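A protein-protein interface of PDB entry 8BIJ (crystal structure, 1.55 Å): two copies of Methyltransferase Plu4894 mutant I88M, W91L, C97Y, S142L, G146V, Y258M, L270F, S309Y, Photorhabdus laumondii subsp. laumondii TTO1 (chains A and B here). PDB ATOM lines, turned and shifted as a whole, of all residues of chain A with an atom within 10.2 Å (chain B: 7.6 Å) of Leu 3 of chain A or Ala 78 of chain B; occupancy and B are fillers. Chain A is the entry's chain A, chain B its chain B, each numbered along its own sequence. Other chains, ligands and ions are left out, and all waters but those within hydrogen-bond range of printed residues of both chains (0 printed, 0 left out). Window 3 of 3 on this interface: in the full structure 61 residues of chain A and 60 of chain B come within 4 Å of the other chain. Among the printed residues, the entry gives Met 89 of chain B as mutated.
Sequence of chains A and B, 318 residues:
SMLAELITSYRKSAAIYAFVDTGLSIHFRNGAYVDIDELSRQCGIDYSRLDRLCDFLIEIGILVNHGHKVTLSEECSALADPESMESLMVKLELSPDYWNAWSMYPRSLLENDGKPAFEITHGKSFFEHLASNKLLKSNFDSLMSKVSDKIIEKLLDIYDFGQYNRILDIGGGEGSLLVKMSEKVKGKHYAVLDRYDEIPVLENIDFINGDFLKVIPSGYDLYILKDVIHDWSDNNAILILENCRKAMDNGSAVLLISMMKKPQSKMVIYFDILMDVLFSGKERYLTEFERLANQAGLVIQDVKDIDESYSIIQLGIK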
ATOM      1  N   SER A   1      24.105 -27.741  20.201  1.00  0.00           N
ATOM      2  CA  SER A   1      24.370 -26.491  20.970  1.00  0.00           C
ATOM      3  C   SER A   1      25.507 -26.737  21.966  1.00  0.00           C
ATOM      4  O   SER A   1      25.620 -27.872  22.475  1.00  0.00           O
ATOM      5  CB  SER A   1      23.124 -25.993  21.670  1.00  0.00           C
ATOM      6  OG  SER A   1      22.911 -26.681  22.897  1.00  0.00           O
ATOM      7  N   MET A   2      26.318 -25.708  22.217  1.00  0.00           N
ATOM      8  CA  MET A   2      27.416 -25.719  23.215  1.00  0.00           C
ATOM      9  C   MET A   2      26.873 -26.260  24.548  1.00  0.00           C
ATOM     10  O   MET A   2      27.520 -27.156  25.132  1.00  0.00           O
ATOM     11  CB  MET A   2      27.981 -24.302  23.369  1.00  0.00           C
ATOM     12  CG  MET A   2      29.023 -24.147  24.450  1.00  0.00           C
ATOM     13  SD  MET A   2      28.278 -23.571  25.990  1.00  0.00           S
ATOM     14  CE  MET A   2      29.674 -22.740  26.743  1.00  0.00           C
ATOM     15  N   LEU A   3      25.699 -25.795  24.991  1.00  0.00           N
ATOM     16  CA  LEU A   3      25.144 -26.158  26.323  1.00  0.00           C
ATOM     17  C   LEU A   3      24.750 -27.640  26.349  1.00  0.00           C
ATOM     18  O   LEU A   3      25.112 -28.317  27.328  1.00  0.00           O
ATOM     19  CB  LEU A   3      23.960 -25.257  26.679  1.00  0.00           C
ATOM     20  CG  LEU A   3      23.234 -25.621  27.976  1.00  0.00           C
ATOM     21  CD1 LEU A   3      24.185 -25.630  29.166  1.00  0.00           C
ATOM     22  CD2 LEU A   3      22.075 -24.672  28.224  1.00  0.00           C
ATOM     23  N   ALA A   4      24.038 -28.129  25.328  1.00  0.00           N
ATOM     24  CA  ALA A   4      23.605 -29.544  25.235  1.00  0.00           C
ATOM     25  C   ALA A   4      24.842 -30.453  25.261  1.00  0.00           C
ATOM     26  O   ALA A   4      24.806 -31.489  25.954  1.00  0.00           O
ATOM     27  CB  ALA A   4      22.764 -29.763  24.001  1.00  0.00           C
ATOM     28  N   GLU A   5      25.908 -30.063  24.555  1.00  0.00           N
ATOM     29  CA  GLU A   5      27.179 -30.834  24.470  1.00  0.00           C
ATOM     30  C   GLU A   5      27.838 -30.904  25.855  1.00  0.00           C
ATOM     31  O   GLU A   5      28.344 -31.989  26.201  1.00  0.00           O
ATOM     32  CB  GLU A   5      28.107 -30.230  23.416  1.00  0.00           C
ATOM     33  CG  GLU A   5      27.638 -30.494  21.994  1.00  0.00           C
ATOM     34  CD  GLU A   5      28.550 -29.977  20.895  1.00  0.00           C
ATOM     35  OE1 GLU A   5      29.725 -29.673  21.192  1.00  0.00           O
ATOM     36  OE2 GLU A   5      28.084 -29.886  19.740  1.00  0.00           O
ATOM     37  N   LEU A   6      27.834 -29.812  26.628  1.00  0.00           N
ATOM     38  CA  LEU A   6      28.357 -29.824  28.023  1.00  0.00           C
ATOM     39  C   LEU A   6      27.492 -30.770  28.865  1.00  0.00           C
ATOM     40  O   LEU A   6      28.052 -31.576  29.611  1.00  0.00           O
ATOM     41  CB  LEU A   6      28.367 -28.408  28.611  1.00  0.00           C
ATOM     42  CG  LEU A   6      29.442 -27.464  28.073  1.00  0.00           C
ATOM     43  CD1 LEU A   6      29.286 -26.073  28.666  1.00  0.00           C
ATOM     44  CD2 LEU A   6      30.840 -27.995  28.348  1.00  0.00           C
ATOM     45  N   ILE A   7      26.167 -30.709  28.723  1.00  0.00           N
ATOM     46  CA  ILE A   7      25.228 -31.529  29.545  1.00  0.00           C
ATOM     47  C   ILE A   7      25.526 -33.020  29.324  1.00  0.00           C
ATOM     48  O   ILE A   7      25.503 -33.771  30.316  1.00  0.00           O
ATOM     49  CB  ILE A   7      23.762 -31.170  29.236  1.00  0.00           C
ATOM     50  CG1 ILE A   7      23.415 -29.768  29.745  1.00  0.00           C
ATOM     51  CG2 ILE A   7      22.804 -32.224  29.783  1.00  0.00           C
ATOM     52  CD1 ILE A   7      22.143 -29.199  29.152  1.00  0.00           C
ATOM     53  N   THR A   8      25.795 -33.433  28.080  1.00  0.00           N
ATOM     54  CA  THR A   8      25.924 -34.864  27.692  1.00  0.00           C
ATOM     55  C   THR A   8      27.403 -35.292  27.710  1.00  0.00           C
ATOM     56  O   THR A   8      27.659 -36.455  27.329  1.00  0.00           O
ATOM     57  CB  THR A   8      25.219 -35.146  26.355  1.00  0.00           C
ATOM     58  OG1 THR A   8      25.853 -34.426  25.297  1.00  0.00           O
ATOM     59  CG2 THR A   8      23.742 -34.808  26.371  1.00  0.00           C
ATOM     60  N   SER A   9      28.318 -34.424  28.185  1.00  0.00           N
ATOM     61  CA  SER A   9      29.790 -34.648  28.231  1.00  0.00           C
ATOM     62  C   SER A   9      30.109 -35.983  28.918  1.00  0.00           C
ATOM     63  O   SER A   9      31.030 -36.679  28.454  1.00  0.00           O
ATOM     64  CB  SER A   9      30.513 -33.521  28.956  1.00  0.00           C
ATOM     65  OG  SER A   9      30.586 -32.350  28.165  1.00  0.00           O
ATOM     66  N   TYR A  10      29.399 -36.295  30.005  1.00  0.00           N
ATOM     67  CA  TYR A  10      29.648 -37.464  30.894  1.00  0.00           C
ATOM     68  C   TYR A  10      29.677 -38.769  30.086  1.00  0.00           C
ATOM     69  O   TYR A  10      30.364 -39.708  30.498  1.00  0.00           O
ATOM     70  CB  TYR A  10      28.595 -37.543  32.004  1.00  0.00           C
ATOM     71  CG  TYR A  10      27.235 -37.935  31.490  1.00  0.00           C
ATOM     72  CD1 TYR A  10      26.385 -36.988  30.943  1.00  0.00           C
ATOM     73  CD2 TYR A  10      26.821 -39.258  31.486  1.00  0.00           C
ATOM     74  CE1 TYR A  10      25.152 -37.346  30.422  1.00  0.00           C
ATOM     75  CE2 TYR A  10      25.583 -39.630  30.975  1.00  0.00           C
ATOM     76  CZ  TYR A  10      24.745 -38.666  30.446  1.00  0.00           C
ATOM     77  OH  TYR A  10      23.519 -38.990  29.909  1.00  0.00           O
ATOM     78  N   LYS A  12      31.070 -39.409  27.294  1.00  0.00           N
ATOM     79  CA  LYS A  12      32.453 -39.565  26.777  1.00  0.00           C
ATOM     80  C   LYS A  12      33.272 -40.330  27.826  1.00  0.00           C
ATOM     81  O   LYS A  12      33.873 -41.369  27.490  1.00  0.00           O
ATOM     82  CB  LYS A  12      33.074 -38.197  26.470  1.00  0.00           C
ATOM     83  CG  LYS A  12      32.386 -37.380  25.382  1.00  0.00           C
ATOM     84  CD  LYS A  12      32.950 -35.980  25.258  1.00  0.00           C
ATOM     85  CE  LYS A  12      32.253 -35.113  24.232  1.00  0.00           C
ATOM     86  NZ  LYS A  12      32.963 -33.824  24.064  1.00  0.00           N
ATOM     87  N   ILE B  16      26.936 -28.944  36.278  1.00  0.00           N
ATOM     88  CA  ILE B  16      25.709 -28.337  35.683  1.00  0.00           C
ATOM     89  C   ILE B  16      24.487 -28.880  36.438  1.00  0.00           C
ATOM     90  O   ILE B  16      23.620 -28.068  36.819  1.00  0.00           O
ATOM     91  CB  ILE B  16      25.677 -28.600  34.169  1.00  0.00           C
ATOM     92  CG1 ILE B  16      26.779 -27.811  33.454  1.00  0.00           C
ATOM     93  CG2 ILE B  16      24.296 -28.290  33.600  1.00  0.00           C
ATOM     94  CD1 ILE B  16      27.103 -28.298  32.065  1.00  0.00           C
ATOM     95  N   VAL B  20      21.700 -26.631  38.756  1.00  0.00           N
ATOM     96  CA  VAL B  20      20.216 -26.662  38.580  1.00  0.00           C
ATOM     97  C   VAL B  20      19.576 -27.272  39.833  1.00  0.00           C
ATOM     98  O   VAL B  20      18.669 -26.635  40.413  1.00  0.00           O
ATOM     99  CB  VAL B  20      19.815 -27.427  37.306  1.00  0.00           C
ATOM    100  CG1 VAL B  20      18.307 -27.580  37.178  1.00  0.00           C
ATOM    101  CG2 VAL B  20      20.392 -26.762  36.065  1.00  0.00           C
ATOM    102  N   SER B  25      20.426 -21.986  39.810  1.00  0.00           N
ATOM    103  CA  SER B  25      20.104 -21.536  38.431  1.00  0.00           C
ATOM    104  C   SER B  25      18.953 -20.519  38.447  1.00  0.00           C
ATOM    105  O   SER B  25      18.973 -19.619  37.587  1.00  0.00           O
ATOM    106  CB  SER B  25      19.779 -22.704  37.528  1.00  0.00           C
ATOM    107  OG  SER B  25      18.673 -23.440  38.026  1.00  0.00           O
ATOM    108  N   GLY B  61      32.693 -22.433  30.904  1.00  0.00           N
ATOM    109  CA  GLY B  61      31.955 -21.481  30.045  1.00  0.00           C
ATOM    110  C   GLY B  61      30.468 -21.373  30.359  1.00  0.00           C
ATOM    111  O   GLY B  61      29.745 -20.755  29.545  1.00  0.00           O
ATOM    112  N   ILE B  62      30.004 -21.933  31.478  1.00  0.00           N
ATOM    113  CA  ILE B  62      28.592 -21.798  31.947  1.00  0.00           C
ATOM    114  C   ILE B  62      28.406 -20.385  32.510  1.00  0.00           C
ATOM    115  O   ILE B  62      27.451 -19.715  32.102  1.00  0.00           O
ATOM    116  CB  ILE B  62      28.207 -22.888  32.970  1.00  0.00           C
ATOM    117  CG1 ILE B  62      28.196 -24.287  32.341  1.00  0.00           C
ATOM    118  CG2 ILE B  62      26.883 -22.562  33.648  1.00  0.00           C
ATOM    119  CD1 ILE B  62      27.066 -24.552  31.367  1.00  0.00           C
ATOM    120  N   LEU B  72      25.166 -15.767  34.103  1.00  0.00           N
ATOM    121  CA  LEU B  72      25.009 -16.955  33.235  1.00  0.00           C
ATOM    122  C   LEU B  72      25.375 -16.533  31.810  1.00  0.00           C
ATOM    123  O   LEU B  72      24.822 -15.523  31.337  1.00  0.00           O
ATOM    124  CB  LEU B  72      23.557 -17.437  33.335  1.00  0.00           C
ATOM    125  CG  LEU B  72      23.202 -18.722  32.591  1.00  0.00           C
ATOM    126  CD1 LEU B  72      24.116 -19.873  32.983  1.00  0.00           C
ATOM    127  CD2 LEU B  72      21.749 -19.088  32.851  1.00  0.00           C
ATOM    128  N   SER B  73      26.300 -17.252  31.173  1.00  0.00           N
ATOM    129  CA  SER B  73      26.689 -17.035  29.758  1.00  0.00           C
ATOM    130  C   SER B  73      25.410 -16.977  28.922  1.00  0.00           C
ATOM    131  O   SER B  73      24.507 -17.802  29.164  1.00  0.00           O
ATOM    132  CB  SER B  73      27.621 -18.108  29.274  1.00  0.00           C
ATOM    133  OG  SER B  73      27.875 -17.956  27.889  1.00  0.00           O
ATOM    134  N   GLU B  74      25.316 -16.025  27.998  1.00  0.00           N
ATOM    135  CA  GLU B  74      24.105 -15.870  27.144  1.00  0.00           C
ATOM    136  C   GLU B  74      23.908 -17.141  26.302  1.00  0.00           C
ATOM    137  O   GLU B  74      22.750 -17.482  26.043  1.00  0.00           O
ATOM    138  CB  GLU B  74      24.198 -14.585  26.326  1.00  0.00           C
ATOM    139  CG  GLU B  74      24.097 -13.339  27.190  1.00  0.00           C
ATOM    140  CD  GLU B  74      24.101 -12.024  26.430  1.00  0.00           C
ATOM    141  OE1 GLU B  74      23.337 -11.908  25.467  1.00  0.00           O
ATOM    142  OE2 GLU B  74      24.888 -11.127  26.797  1.00  0.00           O
ATOM    143  N   GLU B  75      24.986 -17.850  25.955  1.00  0.00           N
ATOM    144  CA  GLU B  75      24.956 -19.173  25.266  1.00  0.00           C
ATOM    145  C   GLU B  75      24.234 -20.225  26.116  1.00  0.00           C
ATOM    146  O   GLU B  75      23.758 -21.214  25.536  1.00  0.00           O
ATOM    147  CB  GLU B  75      26.358 -19.734  25.042  1.00  0.00           C
ATOM    148  CG  GLU B  75      27.263 -18.840  24.234  1.00  0.00           C
ATOM    149  CD  GLU B  75      28.505 -19.561  23.758  1.00  0.00           C
ATOM    150  OE1 GLU B  75      28.352 -20.587  23.062  1.00  0.00           O
ATOM    151  OE2 GLU B  75      29.616 -19.113  24.106  1.00  0.00           O
ATOM    152  N   CYS B  76      24.202 -20.048  27.437  1.00  0.00           N
ATOM    153  CA  CYS B  76      23.705 -21.066  28.401  1.00  0.00           C
ATOM    154  C   CYS B  76      22.480 -20.546  29.163  1.00  0.00           C
ATOM    155  O   CYS B  76      22.129 -21.155  30.191  1.00  0.00           O
ATOM    156  CB  CYS B  76      24.824 -21.460  29.361  1.00  0.00           C
ATOM    157  SG  CYS B  76      26.275 -22.138  28.511  1.00  0.00           S
ATOM    158  N   SER B  77      21.820 -19.505  28.644  1.00  0.00           N
ATOM    159  CA  SER B  77      20.642 -18.852  29.276  1.00  0.00           C
ATOM    160  C   SER B  77      19.551 -19.885  29.590  1.00  0.00           C
ATOM    161  O   SER B  77      18.826 -19.687  30.579  1.00  0.00           O
ATOM    162  CB  SER B  77      20.097 -17.747  28.403  1.00  0.00           C
ATOM    163  OG  SER B  77      20.971 -16.628  28.397  1.00  0.00           O
ATOM    164  N   ALA B  78      19.444 -20.937  28.770  1.00  0.00           N
ATOM    165  CA  ALA B  78      18.417 -22.000  28.896  1.00  0.00           C
ATOM    166  C   ALA B  78      18.443 -22.641  30.293  1.00  0.00           C
ATOM    167  O   ALA B  78      17.388 -23.141  30.720  1.00  0.00           O
ATOM    168  CB  ALA B  78      18.598 -23.031  27.811  1.00  0.00           C
ATOM    169  N   LEU B  79      19.586 -22.640  30.992  1.00  0.00           N
ATOM    170  CA  LEU B  79      19.721 -23.284  32.329  1.00  0.00           C
ATOM    171  C   LEU B  79      18.917 -22.529  33.398  1.00  0.00           C
ATOM    172  O   LEU B  79      18.656 -23.132  34.460  1.00  0.00           O
ATOM    173  CB  LEU B  79      21.198 -23.350  32.726  1.00  0.00           C
ATOM    174  CG  LEU B  79      22.056 -24.396  32.015  1.00  0.00           C
ATOM    175  CD1 LEU B  79      23.450 -24.421  32.624  1.00  0.00           C
ATOM    176  CD2 LEU B  79      21.426 -25.779  32.079  1.00  0.00           C
ATOM    177  N   ALA B  80      18.552 -21.265  33.148  1.00  0.00           N
ATOM    178  CA  ALA B  80      17.735 -20.435  34.066  1.00  0.00           C
ATOM    179  C   ALA B  80      16.247 -20.552  33.700  1.00  0.00           C
ATOM    180  O   ALA B  80      15.421 -19.939  34.403  1.00  0.00           O
ATOM    181  CB  ALA B  80      18.217 -19.004  34.026  1.00  0.00           C
ATOM    182  N   ASP B  81      15.919 -21.311  32.649  1.00  0.00           N
ATOM    183  CA  ASP B  81      14.533 -21.541  32.157  1.00  0.00           C
ATOM    184  C   ASP B  81      14.142 -22.988  32.454  1.00  0.00           C
ATOM    185  O   ASP B  81      14.568 -23.903  31.746  1.00  0.00           O
ATOM    186  CB  ASP B  81      14.437 -21.221  30.662  1.00  0.00           C
ATOM    187  CG  ASP B  81      13.078 -21.481  30.034  1.00  0.00           C
ATOM    188  OD1 ASP B  81      12.122 -21.804  30.775  1.00  0.00           O
ATOM    189  OD2 ASP B  81      12.985 -21.358  28.799  1.00  0.00           O
ATOM    190  N   PRO B  82      13.315 -23.255  33.494  1.00  0.00           N
ATOM    191  CA  PRO B  82      13.032 -24.630  33.910  1.00  0.00           C
ATOM    192  C   PRO B  82      12.316 -25.469  32.840  1.00  0.00           C
ATOM    193  O   PRO B  82      12.391 -26.681  32.918  1.00  0.00           O
ATOM    194  CB  PRO B  82      12.138 -24.480  35.152  1.00  0.00           C
ATOM    195  CG  PRO B  82      12.339 -23.046  35.600  1.00  0.00           C
ATOM    196  CD  PRO B  82      12.616 -22.269  34.331  1.00  0.00           C
ATOM    197  N   GLU B  83      11.656 -24.812  31.879  1.00  0.00           N
ATOM    198  CA  GLU B  83      10.865 -25.480  30.813  1.00  0.00           C
ATOM    199  C   GLU B  83      11.705 -25.611  29.536  1.00  0.00           C
ATOM    200  O   GLU B  83      11.190 -26.192  28.571  1.00  0.00           O
ATOM    201  CB  GLU B  83       9.557 -24.727  30.546  1.00  0.00           C
ATOM    202  CG  GLU B  83       8.620 -24.688  31.744  1.00  0.00           C
ATOM    203  CD  GLU B  83       8.957 -23.662  32.818  1.00  0.00           C
ATOM    204  OE1 GLU B  83       9.456 -22.566  32.461  1.00  0.00           O
ATOM    205  OE2 GLU B  83       8.709 -23.960  34.016  1.00  0.00           O
ATOM    206  N   SER B  84      12.955 -25.133  29.520  1.00  0.00           N
ATOM    207  CA  SER B  84      13.854 -25.302  28.347  1.00  0.00           C
ATOM    208  C   SER B  84      14.166 -26.793  28.181  1.00  0.00           C
ATOM    209  O   SER B  84      14.178 -27.515  29.199  1.00  0.00           O
ATOM    210  CB  SER B  84      15.105 -24.473  28.462  1.00  0.00           C
ATOM    211  OG  SER B  84      16.029 -25.061  29.371  1.00  0.00           O
ATOM    212  N   MET B  85      14.381 -27.242  26.944  1.00  0.00           N
ATOM    213  CA  MET B  85      14.773 -28.644  26.642  1.00  0.00           C
ATOM    214  C   MET B  85      16.019 -28.985  27.473  1.00  0.00           C
ATOM    215  O   MET B  85      16.049 -30.064  28.096  1.00  0.00           O
ATOM    216  CB  MET B  85      15.067 -28.813  25.147  1.00  0.00           C
ATOM    217  CG  MET B  85      15.296 -30.251  24.721  1.00  0.00           C
ATOM    218  SD  MET B  85      13.833 -31.288  24.945  1.00  0.00           S
ATOM    219  CE  MET B  85      12.853 -30.779  23.535  1.00  0.00           C
ATOM    220  N   GLU B  86      16.977 -28.062  27.528  1.00  0.00           N
ATOM    221  CA  GLU B  86      18.276 -28.282  28.218  1.00  0.00           C
ATOM    222  C   GLU B  86      18.031 -28.515  29.714  1.00  0.00           C
ATOM    223  O   GLU B  86      18.594 -29.492  30.251  1.00  0.00           O
ATOM    224  CB  GLU B  86      19.226 -27.114  27.964  1.00  0.00           C
ATOM    225  CG  GLU B  86      19.718 -27.044  26.530  1.00  0.00           C
ATOM    226  CD  GLU B  86      18.894 -26.171  25.599  1.00  0.00           C
ATOM    227  OE1 GLU B  86      17.762 -25.776  25.974  1.00  0.00           O
ATOM    228  OE2 GLU B  86      19.390 -25.880  24.494  1.00  0.00           O
ATOM    229  N   SER B  87      17.231 -27.668  30.372  1.00  0.00           N
ATOM    230  CA  SER B  87      16.915 -27.804  31.821  1.00  0.00           C
ATOM    231  C   SER B  87      16.210 -29.141  32.075  1.00  0.00           C
ATOM    232  O   SER B  87      16.540 -29.794  33.076  1.00  0.00           O
ATOM    233  CB  SER B  87      16.097 -26.652  32.338  1.00  0.00           C
ATOM    234  OG  SER B  87      16.870 -25.466  32.383  1.00  0.00           O
ATOM    235  N   LEU B  88      15.255 -29.523  31.215  1.00  0.00           N
ATOM    236  CA  LEU B  88      14.510 -30.805  31.352  1.00  0.00           C
ATOM    237  C   LEU B  88      15.482 -31.989  31.180  1.00  0.00           C
ATOM    238  O   LEU B  88      15.338 -32.982  31.914  1.00  0.00           O
ATOM    239  CB  LEU B  88      13.357 -30.843  30.340  1.00  0.00           C
ATOM    240  CG  LEU B  88      12.258 -29.796  30.553  1.00  0.00           C
ATOM    241  CD1 LEU B  88      11.268 -29.790  29.397  1.00  0.00           C
ATOM    242  CD2 LEU B  88      11.528 -30.011  31.870  1.00  0.00           C
ATOM    243  N   MET B  89      16.448 -31.890  30.262  1.00  0.00           N
ATOM    244  CA  MET B  89      17.482 -32.938  30.041  1.00  0.00           C
ATOM    245  C   MET B  89      18.333 -33.080  31.315  1.00  0.00           C
ATOM    246  O   MET B  89      18.524 -34.210  31.791  1.00  0.00           O
ATOM    247  CB  MET B  89      18.404 -32.582  28.870  1.00  0.00           C
ATOM    248  CG  MET B  89      17.799 -32.809  27.500  1.00  0.00           C
ATOM    249  SD  MET B  89      18.773 -32.012  26.193  1.00  0.00           S
ATOM    250  CE  MET B  89      20.389 -32.749  26.453  1.00  0.00           C
ATOM    251  N   VAL B  90      18.809 -31.963  31.859  1.00  0.00           N
ATOM    252  CA  VAL B  90      19.647 -31.946  33.094  1.00  0.00           C
ATOM    253  C   VAL B  90      18.877 -32.651  34.219  1.00  0.00           C
ATOM    254  O   VAL B  90      19.455 -33.543  34.873  1.00  0.00           O
ATOM    255  CB  VAL B  90      20.053 -30.510  33.478  1.00  0.00           C
ATOM    256  CG1 VAL B  90      20.660 -30.439  34.873  1.00  0.00           C
ATOM    257  CG2 VAL B  90      21.008 -29.917  32.449  1.00  0.00           C
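Of the 24 printed residues of chain B, 10 touch a printed residue of chain A.
Printed residues of chain A that touch a printed residue of chain B: Ser 1, Met 2, Leu 3, Leu 6, Ile 7 and Thr 8.
Hydrophobic or aromatic side chains of chain A within 4 Å of the printed part of chain B: Met 2, Leu 3, Leu 6 and Ile 7.
Among the printed residues, 14 pairs touch across the chains.
The backbone carbonyl oxygen (O) of Ala 4 of chain A lies within hydrogen-bond range of the side-chain hydroxyl (OG1) of Thr 8 of chain A (3.2 Å).
The backbone carbonyl oxygen (O) of Leu 6 of chain A lies within hydrogen-bond range of the side-chain hydroxyl (OG) of Ser 9 of chain A.
O of Ile 62 of chain B is in hydrogen-bond range of N of Ser 73 of chain B, 2.9 Å away.
OG of Ser 73 of chain B sits close to N of Glu 75 of chain B (3.5 Å).
OG of Ser 84 of chain B is in hydrogen-bond range of O of Ala 78 of chain B (2.7 Å).
The backbone carbonyl oxygen (O) of Ala 78 of chain B sits at hydrogen-bond distance from the side-chain hydroxyl (OG) of Ser 87 of chain B.
The side-chain sulfur (SD) of Met 2 of chain A sits at hydrogen-bond distance from the side-chain sulfur (SG) of Cys 76 of chain B (3.5 Å).
Among the printed residues, pairs that only touch across the chains: Ser 1 of chain A with Glu 86 of chain B (3.9 Å), Met 2 of chain A with Gly 61 of chain B (3.4 Å), Met 2 of chain A with Glu 75 of chain B (3.7 Å), Leu 3 of chain A with Ile 62 of chain B (3.8 Å), Leu 3 of chain A with Cys 76 of chain B (3.96 Å), Leu 3 of chain A with Ala 78 of chain B (3.9 Å), Leu 3 of chain A with Leu 79 of chain B (3.7 Å), Leu 3 of chain A with Glu 86 of chain B (3.7 Å), Leu 6 of chain A with Ile 16 of chain B (3.7 Å), Leu 6 of chain A with Ile 62 of chain B (3.8 Å), Ile 7 of chain A with Glu 86 of chain B (3.7 Å), Ile 7 of chain A with Val 90 of chain B (3.6 Å) and Thr 8 of chain A with Met 89 of chain B (3.9 Å).
Of the printed residues of chain B, Leu 3 of chain A touches Ile 62 (3.8 Å), Cys 76 (3.96 Å), Ala 78 (3.9 Å), Leu 79 (3.7 Å) and Glu 86 (3.7 Å).
Ala 78 of chain B touches just one residue of chain A: Leu 3.
Leu 79 of chain B touches just one residue of chain A: Leu 3.
No residue of chain A comes within 4 Å of Ala 80 of chain B.
No residue of chain A comes within 4 Å of Asp 81 of chain B.
No residue of chain A comes within 4 Å of Ser 84 of chain B.
Printed residues of chain B within 4 Å of Ile 7 of chain A: Glu 86 and Val 90.
Printed residues of chain B within 4 Å of Thr 8 of chain A: Met 89 (3.9 Å).
Of the printed residues of chain B, Met 2 of chain A touches Gly 61, Glu 75 and Cys 76.
Printed residues of chain A within 4 Å of Ile 16 of chain B: Leu 6 (3.7 Å).
Printed residues of chain A within 4 Å of Val 90 of chain B: Ile 7 (3.6 Å).
Met 85 of chain B touches none of the printed residues of chain A.
The nearest residue of chain A that does not touch Ala 78 of chain B is Ile 7 of chain A (7.2 Å).
The nearest printed residue of chain B that does not touch Ile 7 of chain A is Met 89 of chain B (4.1 Å).
No position is printed for both chains.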
